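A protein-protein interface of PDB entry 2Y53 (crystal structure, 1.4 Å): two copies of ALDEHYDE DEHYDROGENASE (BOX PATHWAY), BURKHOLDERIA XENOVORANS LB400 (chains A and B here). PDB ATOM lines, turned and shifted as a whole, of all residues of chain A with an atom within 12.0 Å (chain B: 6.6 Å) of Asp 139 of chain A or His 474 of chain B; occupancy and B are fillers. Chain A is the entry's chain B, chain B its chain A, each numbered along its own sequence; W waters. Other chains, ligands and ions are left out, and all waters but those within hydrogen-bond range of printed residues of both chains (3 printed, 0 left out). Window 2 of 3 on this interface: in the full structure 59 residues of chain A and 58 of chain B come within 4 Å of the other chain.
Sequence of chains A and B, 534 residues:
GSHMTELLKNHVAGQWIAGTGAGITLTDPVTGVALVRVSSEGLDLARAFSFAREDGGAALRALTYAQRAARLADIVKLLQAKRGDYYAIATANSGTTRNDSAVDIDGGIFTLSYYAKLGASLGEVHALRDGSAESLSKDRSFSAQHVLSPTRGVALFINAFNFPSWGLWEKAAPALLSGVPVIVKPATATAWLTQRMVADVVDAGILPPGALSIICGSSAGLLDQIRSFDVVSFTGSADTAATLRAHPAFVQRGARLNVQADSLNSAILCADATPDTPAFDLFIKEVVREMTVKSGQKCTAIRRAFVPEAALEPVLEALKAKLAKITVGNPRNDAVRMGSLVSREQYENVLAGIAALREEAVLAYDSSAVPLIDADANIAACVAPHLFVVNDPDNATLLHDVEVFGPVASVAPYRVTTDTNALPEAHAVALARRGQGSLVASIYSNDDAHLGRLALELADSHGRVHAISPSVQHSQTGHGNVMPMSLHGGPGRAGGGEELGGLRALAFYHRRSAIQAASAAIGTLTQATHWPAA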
ATOM      1  N   GLU A 134     -21.027  19.742  19.608  1.00  0.00           N
ATOM      2  CA  GLU A 134     -21.218  18.354  19.367  1.00  0.00           C
ATOM      3  C   GLU A 134     -20.608  17.593  20.528  1.00  0.00           C
ATOM      4  O   GLU A 134     -19.475  17.951  20.980  1.00  0.00           O
ATOM      5  CB  GLU A 134     -20.393  18.043  18.025  1.00  0.00           C
ATOM      6  CG  GLU A 134     -20.372  16.622  17.646  1.00  0.00           C
ATOM      7  CD  GLU A 134     -20.120  16.317  16.118  1.00  0.00           C
ATOM      8  OE1 GLU A 134     -19.995  17.409  15.428  1.00  0.00           O
ATOM      9  OE2 GLU A 134     -20.275  15.199  15.757  1.00  0.00           O
ATOM     10  N   SER A 135     -21.233  16.573  21.058  1.00  0.00           N
ATOM     11  CA  SER A 135     -20.657  15.747  22.121  1.00  0.00           C
ATOM     12  C   SER A 135     -19.607  14.879  21.537  1.00  0.00           C
ATOM     13  O   SER A 135     -19.722  14.325  20.416  1.00  0.00           O
ATOM     14  CB  SER A 135     -21.854  14.885  22.724  1.00  0.00           C
ATOM     15  OG  SER A 135     -21.277  14.081  23.737  1.00  0.00           O
ATOM     16  N   LEU A 136     -18.554  14.712  22.339  1.00  0.00           N
ATOM     17  CA  LEU A 136     -17.450  13.794  22.073  1.00  0.00           C
ATOM     18  C   LEU A 136     -17.397  12.673  23.101  1.00  0.00           C
ATOM     19  O   LEU A 136     -16.439  11.912  23.152  1.00  0.00           O
ATOM     20  CB  LEU A 136     -16.103  14.545  22.032  1.00  0.00           C
ATOM     21  CG  LEU A 136     -15.915  15.611  20.973  1.00  0.00           C
ATOM     22  CD1 LEU A 136     -14.513  16.234  21.084  1.00  0.00           C
ATOM     23  CD2 LEU A 136     -16.080  14.989  19.626  1.00  0.00           C
ATOM     24  N   SER A 137     -18.446  12.463  23.906  1.00  0.00           N
ATOM     25  CA  SER A 137     -18.450  11.447  24.959  1.00  0.00           C
ATOM     26  C   SER A 137     -19.884  10.921  25.167  1.00  0.00           C
ATOM     27  O   SER A 137     -20.816  11.685  25.138  1.00  0.00           O
ATOM     28  CB  SER A 137     -17.990  12.060  26.302  1.00  0.00           C
ATOM     29  OG  SER A 137     -18.610  13.346  26.498  1.00  0.00           O
ATOM     30  N   LYS A 138     -19.997   9.632  25.485  1.00  0.00           N
ATOM     31  CA  LYS A 138     -21.338   9.103  25.864  1.00  0.00           C
ATOM     32  C   LYS A 138     -22.053   9.912  26.949  1.00  0.00           C
ATOM     33  O   LYS A 138     -23.256  10.239  26.829  1.00  0.00           O
ATOM     34  CB  LYS A 138     -21.180   7.611  26.293  1.00  0.00           C
ATOM     35  CG  LYS A 138     -22.541   6.885  26.631  1.00  0.00           C
ATOM     36  CD  LYS A 138     -23.488   6.967  25.380  1.00  0.00           C
ATOM     37  CE  LYS A 138     -24.605   5.888  25.323  1.00  0.00           C
ATOM     38  NZ  LYS A 138     -25.868   6.392  26.018  1.00  0.00           N
ATOM     39  N   ASP A 139     -21.322  10.332  27.967  1.00  0.00           N
ATOM     40  CA  ASP A 139     -21.966  11.080  29.097  1.00  0.00           C
ATOM     41  C   ASP A 139     -22.082  12.537  28.897  1.00  0.00           C
ATOM     42  O   ASP A 139     -22.490  13.261  29.792  1.00  0.00           O
ATOM     43  CB  ASP A 139     -21.292  10.795  30.425  1.00  0.00           C
ATOM     44  CG  ASP A 139     -19.855  11.274  30.493  1.00  0.00           C
ATOM     45  OD1 ASP A 139     -19.364  12.028  29.622  1.00  0.00           O
ATOM     46  OD2 ASP A 139     -19.258  11.066  31.574  1.00  0.00           O
ATOM     47  N   ARG A 140     -21.686  13.014  27.697  1.00  0.00           N
ATOM     48  CA  ARG A 140     -21.748  14.465  27.321  1.00  0.00           C
ATOM     49  C   ARG A 140     -20.928  15.386  28.191  1.00  0.00           C
ATOM     50  O   ARG A 140     -21.074  16.612  28.204  1.00  0.00           O
ATOM     51  CB  ARG A 140     -23.227  14.971  27.313  1.00  0.00           C
ATOM     52  CG  ARG A 140     -24.138  14.165  26.341  1.00  0.00           C
ATOM     53  CD  ARG A 140     -25.592  14.818  26.315  1.00  0.00           C
ATOM     54  NE  ARG A 140     -25.475  16.213  25.840  1.00  0.00           N
ATOM     55  CZ  ARG A 140     -25.585  16.558  24.541  1.00  0.00           C
ATOM     56  NH1 ARG A 140     -25.816  15.635  23.623  1.00  0.00           N
ATOM     57  NH2 ARG A 140     -25.440  17.815  24.161  1.00  0.00           N
ATOM     58  N   SER A 141     -19.942  14.833  28.879  1.00  0.00           N
ATOM     59  CA  SER A 141     -19.045  15.610  29.712  1.00  0.00           C
ATOM     60  C   SER A 141     -17.976  16.339  28.876  1.00  0.00           C
ATOM     61  O   SER A 141     -17.480  17.358  29.332  1.00  0.00           O
ATOM     62  CB  SER A 141     -18.326  14.784  30.817  1.00  0.00           C
ATOM     63  OG  SER A 141     -17.530  13.755  30.255  1.00  0.00           O
ATOM     64  N   PHE A 142     -17.643  15.757  27.697  1.00  0.00           N
ATOM     65  CA  PHE A 142     -16.584  16.406  26.839  1.00  0.00           C
ATOM     66  C   PHE A 142     -17.240  16.633  25.492  1.00  0.00           C
ATOM     67  O   PHE A 142     -17.876  15.736  24.935  1.00  0.00           O
ATOM     68  CB  PHE A 142     -15.458  15.364  26.723  1.00  0.00           C
ATOM     69  CG  PHE A 142     -14.181  15.933  26.073  1.00  0.00           C
ATOM     70  CD1 PHE A 142     -13.454  16.876  26.738  1.00  0.00           C
ATOM     71  CD2 PHE A 142     -13.745  15.460  24.807  1.00  0.00           C
ATOM     72  CE1 PHE A 142     -12.254  17.409  26.238  1.00  0.00           C
ATOM     73  CE2 PHE A 142     -12.558  15.998  24.274  1.00  0.00           C
ATOM     74  CZ  PHE A 142     -11.819  16.917  24.947  1.00  0.00           C
ATOM     75  N   SER A 143     -17.106  17.896  24.994  1.00  0.00           N
ATOM     76  CA  SER A 143     -17.758  18.332  23.736  1.00  0.00           C
ATOM     77  C   SER A 143     -16.847  19.181  22.912  1.00  0.00           C
ATOM     78  O   SER A 143     -15.739  19.545  23.336  1.00  0.00           O
ATOM     79  CB  SER A 143     -19.000  19.261  24.079  1.00  0.00           C
ATOM     80  OG  SER A 143     -19.985  18.360  24.622  1.00  0.00           O
ATOM     81  N   ALA A 144     -17.277  19.482  21.700  1.00  0.00           N
ATOM     82  CA  ALA A 144     -16.462  20.312  20.768  1.00  0.00           C
ATOM     83  C   ALA A 144     -17.280  21.393  20.170  1.00  0.00           C
ATOM     84  O   ALA A 144     -18.426  21.139  19.817  1.00  0.00           O
ATOM     85  CB  ALA A 144     -15.908  19.405  19.648  1.00  0.00           C
ATOM     86  N   ALA A 517     -13.469  20.445  24.886  1.00  0.00           N
ATOM     87  CA  ALA A 517     -13.320  20.796  26.299  1.00  0.00           C
ATOM     88  C   ALA A 517     -14.516  20.175  27.067  1.00  0.00           C
ATOM     89  O   ALA A 517     -15.505  19.779  26.543  1.00  0.00           O
ATOM     90  CB  ALA A 517     -13.262  22.339  26.510  1.00  0.00           C
ATOM     91  N   ALA A 518     -14.344  20.312  28.387  1.00  0.00           N
ATOM     92  CA  ALA A 518     -15.465  20.097  29.306  1.00  0.00           C
ATOM     93  C   ALA A 518     -16.649  20.870  28.788  1.00  0.00           C
ATOM     94  O   ALA A 518     -16.560  22.025  28.399  1.00  0.00           O
ATOM     95  CB  ALA A 518     -15.104  20.629  30.713  1.00  0.00           C
ATOM     96  N   SER A 519     -17.799  20.241  28.881  1.00  0.00           N
ATOM     97  CA  SER A 519     -19.044  20.830  28.363  1.00  0.00           C
ATOM     98  C   SER A 519     -19.392  22.207  28.995  1.00  0.00           C
ATOM     99  O   SER A 519     -19.876  23.112  28.237  1.00  0.00           O
ATOM    100  CB  SER A 519     -20.219  19.787  28.344  1.00  0.00           C
ATOM    101  OG  SER A 519     -19.916  18.671  27.456  1.00  0.00           O
ATOM    102  N   ALA A 520     -19.028  22.428  30.254  1.00  0.00           N
ATOM    103  CA  ALA A 520     -19.287  23.794  30.869  1.00  0.00           C
ATOM    104  C   ALA A 520     -18.504  24.867  30.129  1.00  0.00           C
ATOM    105  O   ALA A 520     -19.121  25.927  29.757  1.00  0.00           O
ATOM    106  CB  ALA A 520     -18.999  23.796  32.434  1.00  0.00           C
ATOM    107  N   ILE A 522     -17.374  24.743  27.053  1.00  0.00           N
ATOM    108  CA  ILE A 522     -17.962  24.921  25.712  1.00  0.00           C
ATOM    109  C   ILE A 522     -19.172  25.857  25.836  1.00  0.00           C
ATOM    110  O   ILE A 522     -19.471  26.582  24.900  1.00  0.00           O
ATOM    111  CB  ILE A 522     -18.339  23.579  25.058  1.00  0.00           C
ATOM    112  CG1 ILE A 522     -17.041  22.702  24.794  1.00  0.00           C
ATOM    113  CG2 ILE A 522     -19.101  23.760  23.722  1.00  0.00           C
ATOM    114  CD1 ILE A 522     -15.965  23.355  23.889  1.00  0.00           C
ATOM    115  N   SER B 469      -9.189  18.596  31.961  1.00  0.00           N
ATOM    116  CA  SER B 469      -9.481  19.010  33.334  1.00  0.00           C
ATOM    117  C   SER B 469     -10.132  17.789  34.007  1.00  0.00           C
ATOM    118  O   SER B 469     -10.488  16.838  33.386  1.00  0.00           O
ATOM    119  CB  SER B 469     -10.393  20.232  33.322  1.00  0.00           C
ATOM    120  OG  SER B 469     -11.607  19.890  32.628  1.00  0.00           O
ATOM    121  N   PRO B 470     -10.161  17.886  35.370  1.00  0.00           N
ATOM    122  CA  PRO B 470     -10.674  16.719  36.069  1.00  0.00           C
ATOM    123  C   PRO B 470     -12.060  16.197  35.679  1.00  0.00           C
ATOM    124  O   PRO B 470     -12.268  14.972  35.670  1.00  0.00           O
ATOM    125  CB  PRO B 470     -10.603  17.173  37.538  1.00  0.00           C
ATOM    126  CG  PRO B 470      -9.403  18.182  37.566  1.00  0.00           C
ATOM    127  CD  PRO B 470      -9.603  18.927  36.260  1.00  0.00           C
ATOM    128  N   SER B 471     -12.961  17.128  35.344  1.00  0.00           N
ATOM    129  CA  SER B 471     -14.264  16.634  35.007  1.00  0.00           C
ATOM    130  C   SER B 471     -14.351  15.786  33.728  1.00  0.00           C
ATOM    131  O   SER B 471     -15.323  15.166  33.436  1.00  0.00           O
ATOM    132  CB  SER B 471     -15.250  17.766  34.858  1.00  0.00           C
ATOM    133  OG  SER B 471     -15.043  18.596  33.645  1.00  0.00           O
ATOM    134  N   VAL B 472     -13.276  15.849  32.910  1.00  0.00           N
ATOM    135  CA  VAL B 472     -13.185  15.062  31.691  1.00  0.00           C
ATOM    136  C   VAL B 472     -11.987  14.112  31.740  1.00  0.00           C
ATOM    137  O   VAL B 472     -11.518  13.608  30.708  1.00  0.00           O
ATOM    138  CB  VAL B 472     -13.106  16.005  30.445  1.00  0.00           C
ATOM    139  CG1 VAL B 472     -14.419  16.804  30.386  1.00  0.00           C
ATOM    140  CG2 VAL B 472     -11.848  16.942  30.456  1.00  0.00           C
ATOM    141  N   GLN B 473     -11.524  13.757  32.941  1.00  0.00           N
ATOM    142  CA  GLN B 473     -10.396  12.830  33.020  1.00  0.00           C
ATOM    143  C   GLN B 473     -10.679  11.489  32.331  1.00  0.00           C
ATOM    144  O   GLN B 473      -9.826  10.867  31.700  1.00  0.00           O
ATOM    145  CB  GLN B 473     -10.009  12.676  34.498  1.00  0.00           C
ATOM    146  CG  GLN B 473     -10.915  11.904  35.294  1.00  0.00           C
ATOM    147  CD  GLN B 473     -10.392  11.701  36.724  1.00  0.00           C
ATOM    148  OE1 GLN B 473      -9.169  11.566  36.949  1.00  0.00           O
ATOM    149  NE2 GLN B 473     -11.345  11.675  37.708  1.00  0.00           N
ATOM    150  N   HIS B 474     -11.916  11.053  32.389  1.00  0.00           N
ATOM    151  CA  HIS B 474     -12.287   9.773  31.852  1.00  0.00           C
ATOM    152  C   HIS B 474     -12.915   9.875  30.427  1.00  0.00           C
ATOM    153  O   HIS B 474     -13.162   8.873  29.761  1.00  0.00           O
ATOM    154  CB  HIS B 474     -13.441   9.247  32.766  1.00  0.00           C
ATOM    155  CG  HIS B 474     -14.674  10.142  32.677  1.00  0.00           C
ATOM    156  ND1 HIS B 474     -14.721  11.537  32.974  1.00  0.00           N
ATOM    157  CD2 HIS B 474     -15.897   9.835  32.150  1.00  0.00           C
ATOM    158  CE1 HIS B 474     -15.947  11.965  32.707  1.00  0.00           C
ATOM    159  NE2 HIS B 474     -16.644  10.975  32.151  1.00  0.00           N
ATOM    160  N   SER B 475     -13.135  11.092  29.933  1.00  0.00           N
ATOM    161  CA  SER B 475     -13.864  11.276  28.641  1.00  0.00           C
ATOM    162  C   SER B 475     -13.058  12.058  27.571  1.00  0.00           C
ATOM    163  O   SER B 475     -13.401  11.991  26.419  1.00  0.00           O
ATOM    164  CB  SER B 475     -15.189  12.032  28.871  1.00  0.00           C
ATOM    165  OG  SER B 475     -14.932  13.238  29.527  1.00  0.00           O
ATOM    166  N   GLN B 476     -12.078  12.808  28.019  1.00  0.00           N
ATOM    167  CA  GLN B 476     -11.302  13.638  27.067  1.00  0.00           C
ATOM    168  C   GLN B 476     -10.591  12.661  26.100  1.00  0.00           C
ATOM    169  O   GLN B 476     -10.095  11.599  26.470  1.00  0.00           O
ATOM    170  CB  GLN B 476     -10.328  14.518  27.778  1.00  0.00           C
ATOM    171  CG  GLN B 476      -9.165  13.826  28.511  1.00  0.00           C
ATOM    172  CD  GLN B 476      -7.875  13.660  27.685  1.00  0.00           C
ATOM    173  OE1 GLN B 476      -7.766  14.079  26.540  1.00  0.00           O
ATOM    174  NE2 GLN B 476      -6.879  13.083  28.330  1.00  0.00           N
HETATM  175  O   HOH W   1     -11.756  20.506  29.740  1.00  0.00           O
HETATM  176  O   HOH W   2     -17.330  18.214  32.100  1.00  0.00           O
HETATM  177  O   HOH W   3     -15.048  10.392  25.047  1.00  0.00           O
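No position is printed for both chains.
Of the 10 pairs that touch across the chains among the printed residues, none has its exchanged pair printed and touching as well.
The side-chain hydroxyl (OG) of Ser 137 of chain A lies within hydrogen-bond range of the backbone NH (N) of Phe 142 of chain A (2.9 Å).
N of Ser 141 of chain A lies within hydrogen-bond range of OG of Ser 137 of chain A (3.1 Å).
N of Leu 136 of chain A is in hydrogen-bond range of O of Phe 142 of chain A.
The side-chain hydroxyl of Ser 135 of chain A is in hydrogen-bond range of the backbone carbonyl oxygen of Ser 137 of chain A (2.8 Å).
The backbone carbonyl oxygen of Ser 141 of chain A is in hydrogen-bond range of the backbone NH of Ser 519 of chain A, 2.9 Å away.
OD1 of Asp 139 of chain A is in hydrogen-bond range of OG of Ser 141 of chain A.
Hydrophobic or aromatic side chains of chain A that line the printed part of chain B: Phe 142 and Ala 518.
Among the printed residues, no Asp or Glu carboxylate lies within 4 Å of a Lys or Arg side-chain nitrogen of the other chain.
The side-chain hydroxyl (OG) of Ser 141 of chain A is in hydrogen-bond range of the side-chain hydroxyl (OG) of Ser 475 of chain B.
NE2 of His 474 of chain B sits close to OG of Ser 141 of chain A.
A ring nitrogen (NE2) of His 474 of chain B lies within hydrogen-bond range of the side-chain carboxylate (OD2) of Asp 139 of chain A (2.7 Å).
Ser 135 of chain A touches none of the printed residues of chain B.
Of the printed residues of chain B, Ser 137 of chain A touches Ser 475 (3.8 Å).
Of the printed residues of chain B, Asp 139 of chain A touches His 474.
Printed residues of chain B within 4 Å of Ser 141 of chain A: Val 472 (3.3 Å), His 474 (3.4 Å) and Ser 475 (2.7 Å).
Of the printed residues of chain B, Phe 142 of chain A touches Val 472 (3.8 Å), Ser 475 (3.6 Å) and Gln 476 (3.8 Å).
Ala 144 of chain A touches none of the printed residues of chain B.
Of the printed residues of chain B, Ala 518 of chain A touches Ser 471 and Val 472.
Printed residues of chain A within 4 Å of Ser 471 of chain B: Ala 518 (3.6 Å).
Of chain A, only Asp 139 (2.7 Å) and Ser 141 (3.4 Å) come within 4 Å of His 474 of chain B.
Of chain A, only Ser 137 (3.8 Å), Ser 141 (2.7 Å) and Phe 142 (3.6 Å) come within 4 Å of Ser 475 of chain B.
The nearest residue of chain A that does not touch His 474 of chain B is Ser 137 of chain A (6.1 Å).
Water W3 bridges O of Ser 475 of chain B (2.7 Å) and O of Leu 136 of chain A (2.8 Å).
Water W2 bridges the side-chain hydroxyl of Ser 471 of chain B and the backbone carbonyl oxygen of Ser 141 of chain A.
Water W1 bridges N of Ala 518 of chain A (2.9 Å) and OG of Ser 469 of chain B (3.0 Å).
Among the printed residues, merely in contact across the chains: Ser 137 of chain A with Ser 475 of chain B (3.8 Å), Ser 141 of chain A with Val 472 of chain B (3.3 Å), Phe 142 of chain A with Val 472 of chain B (3.8 Å), Phe 142 of chain A with Ser 475 of chain B (3.6 Å), Phe 142 of chain A with Gln 476 of chain B (3.8 Å), Ala 518 of chain A with Ser 471 of chain B (3.6 Å) and Ala 518 of chain A with Val 472 of chain B (3.6 Å).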
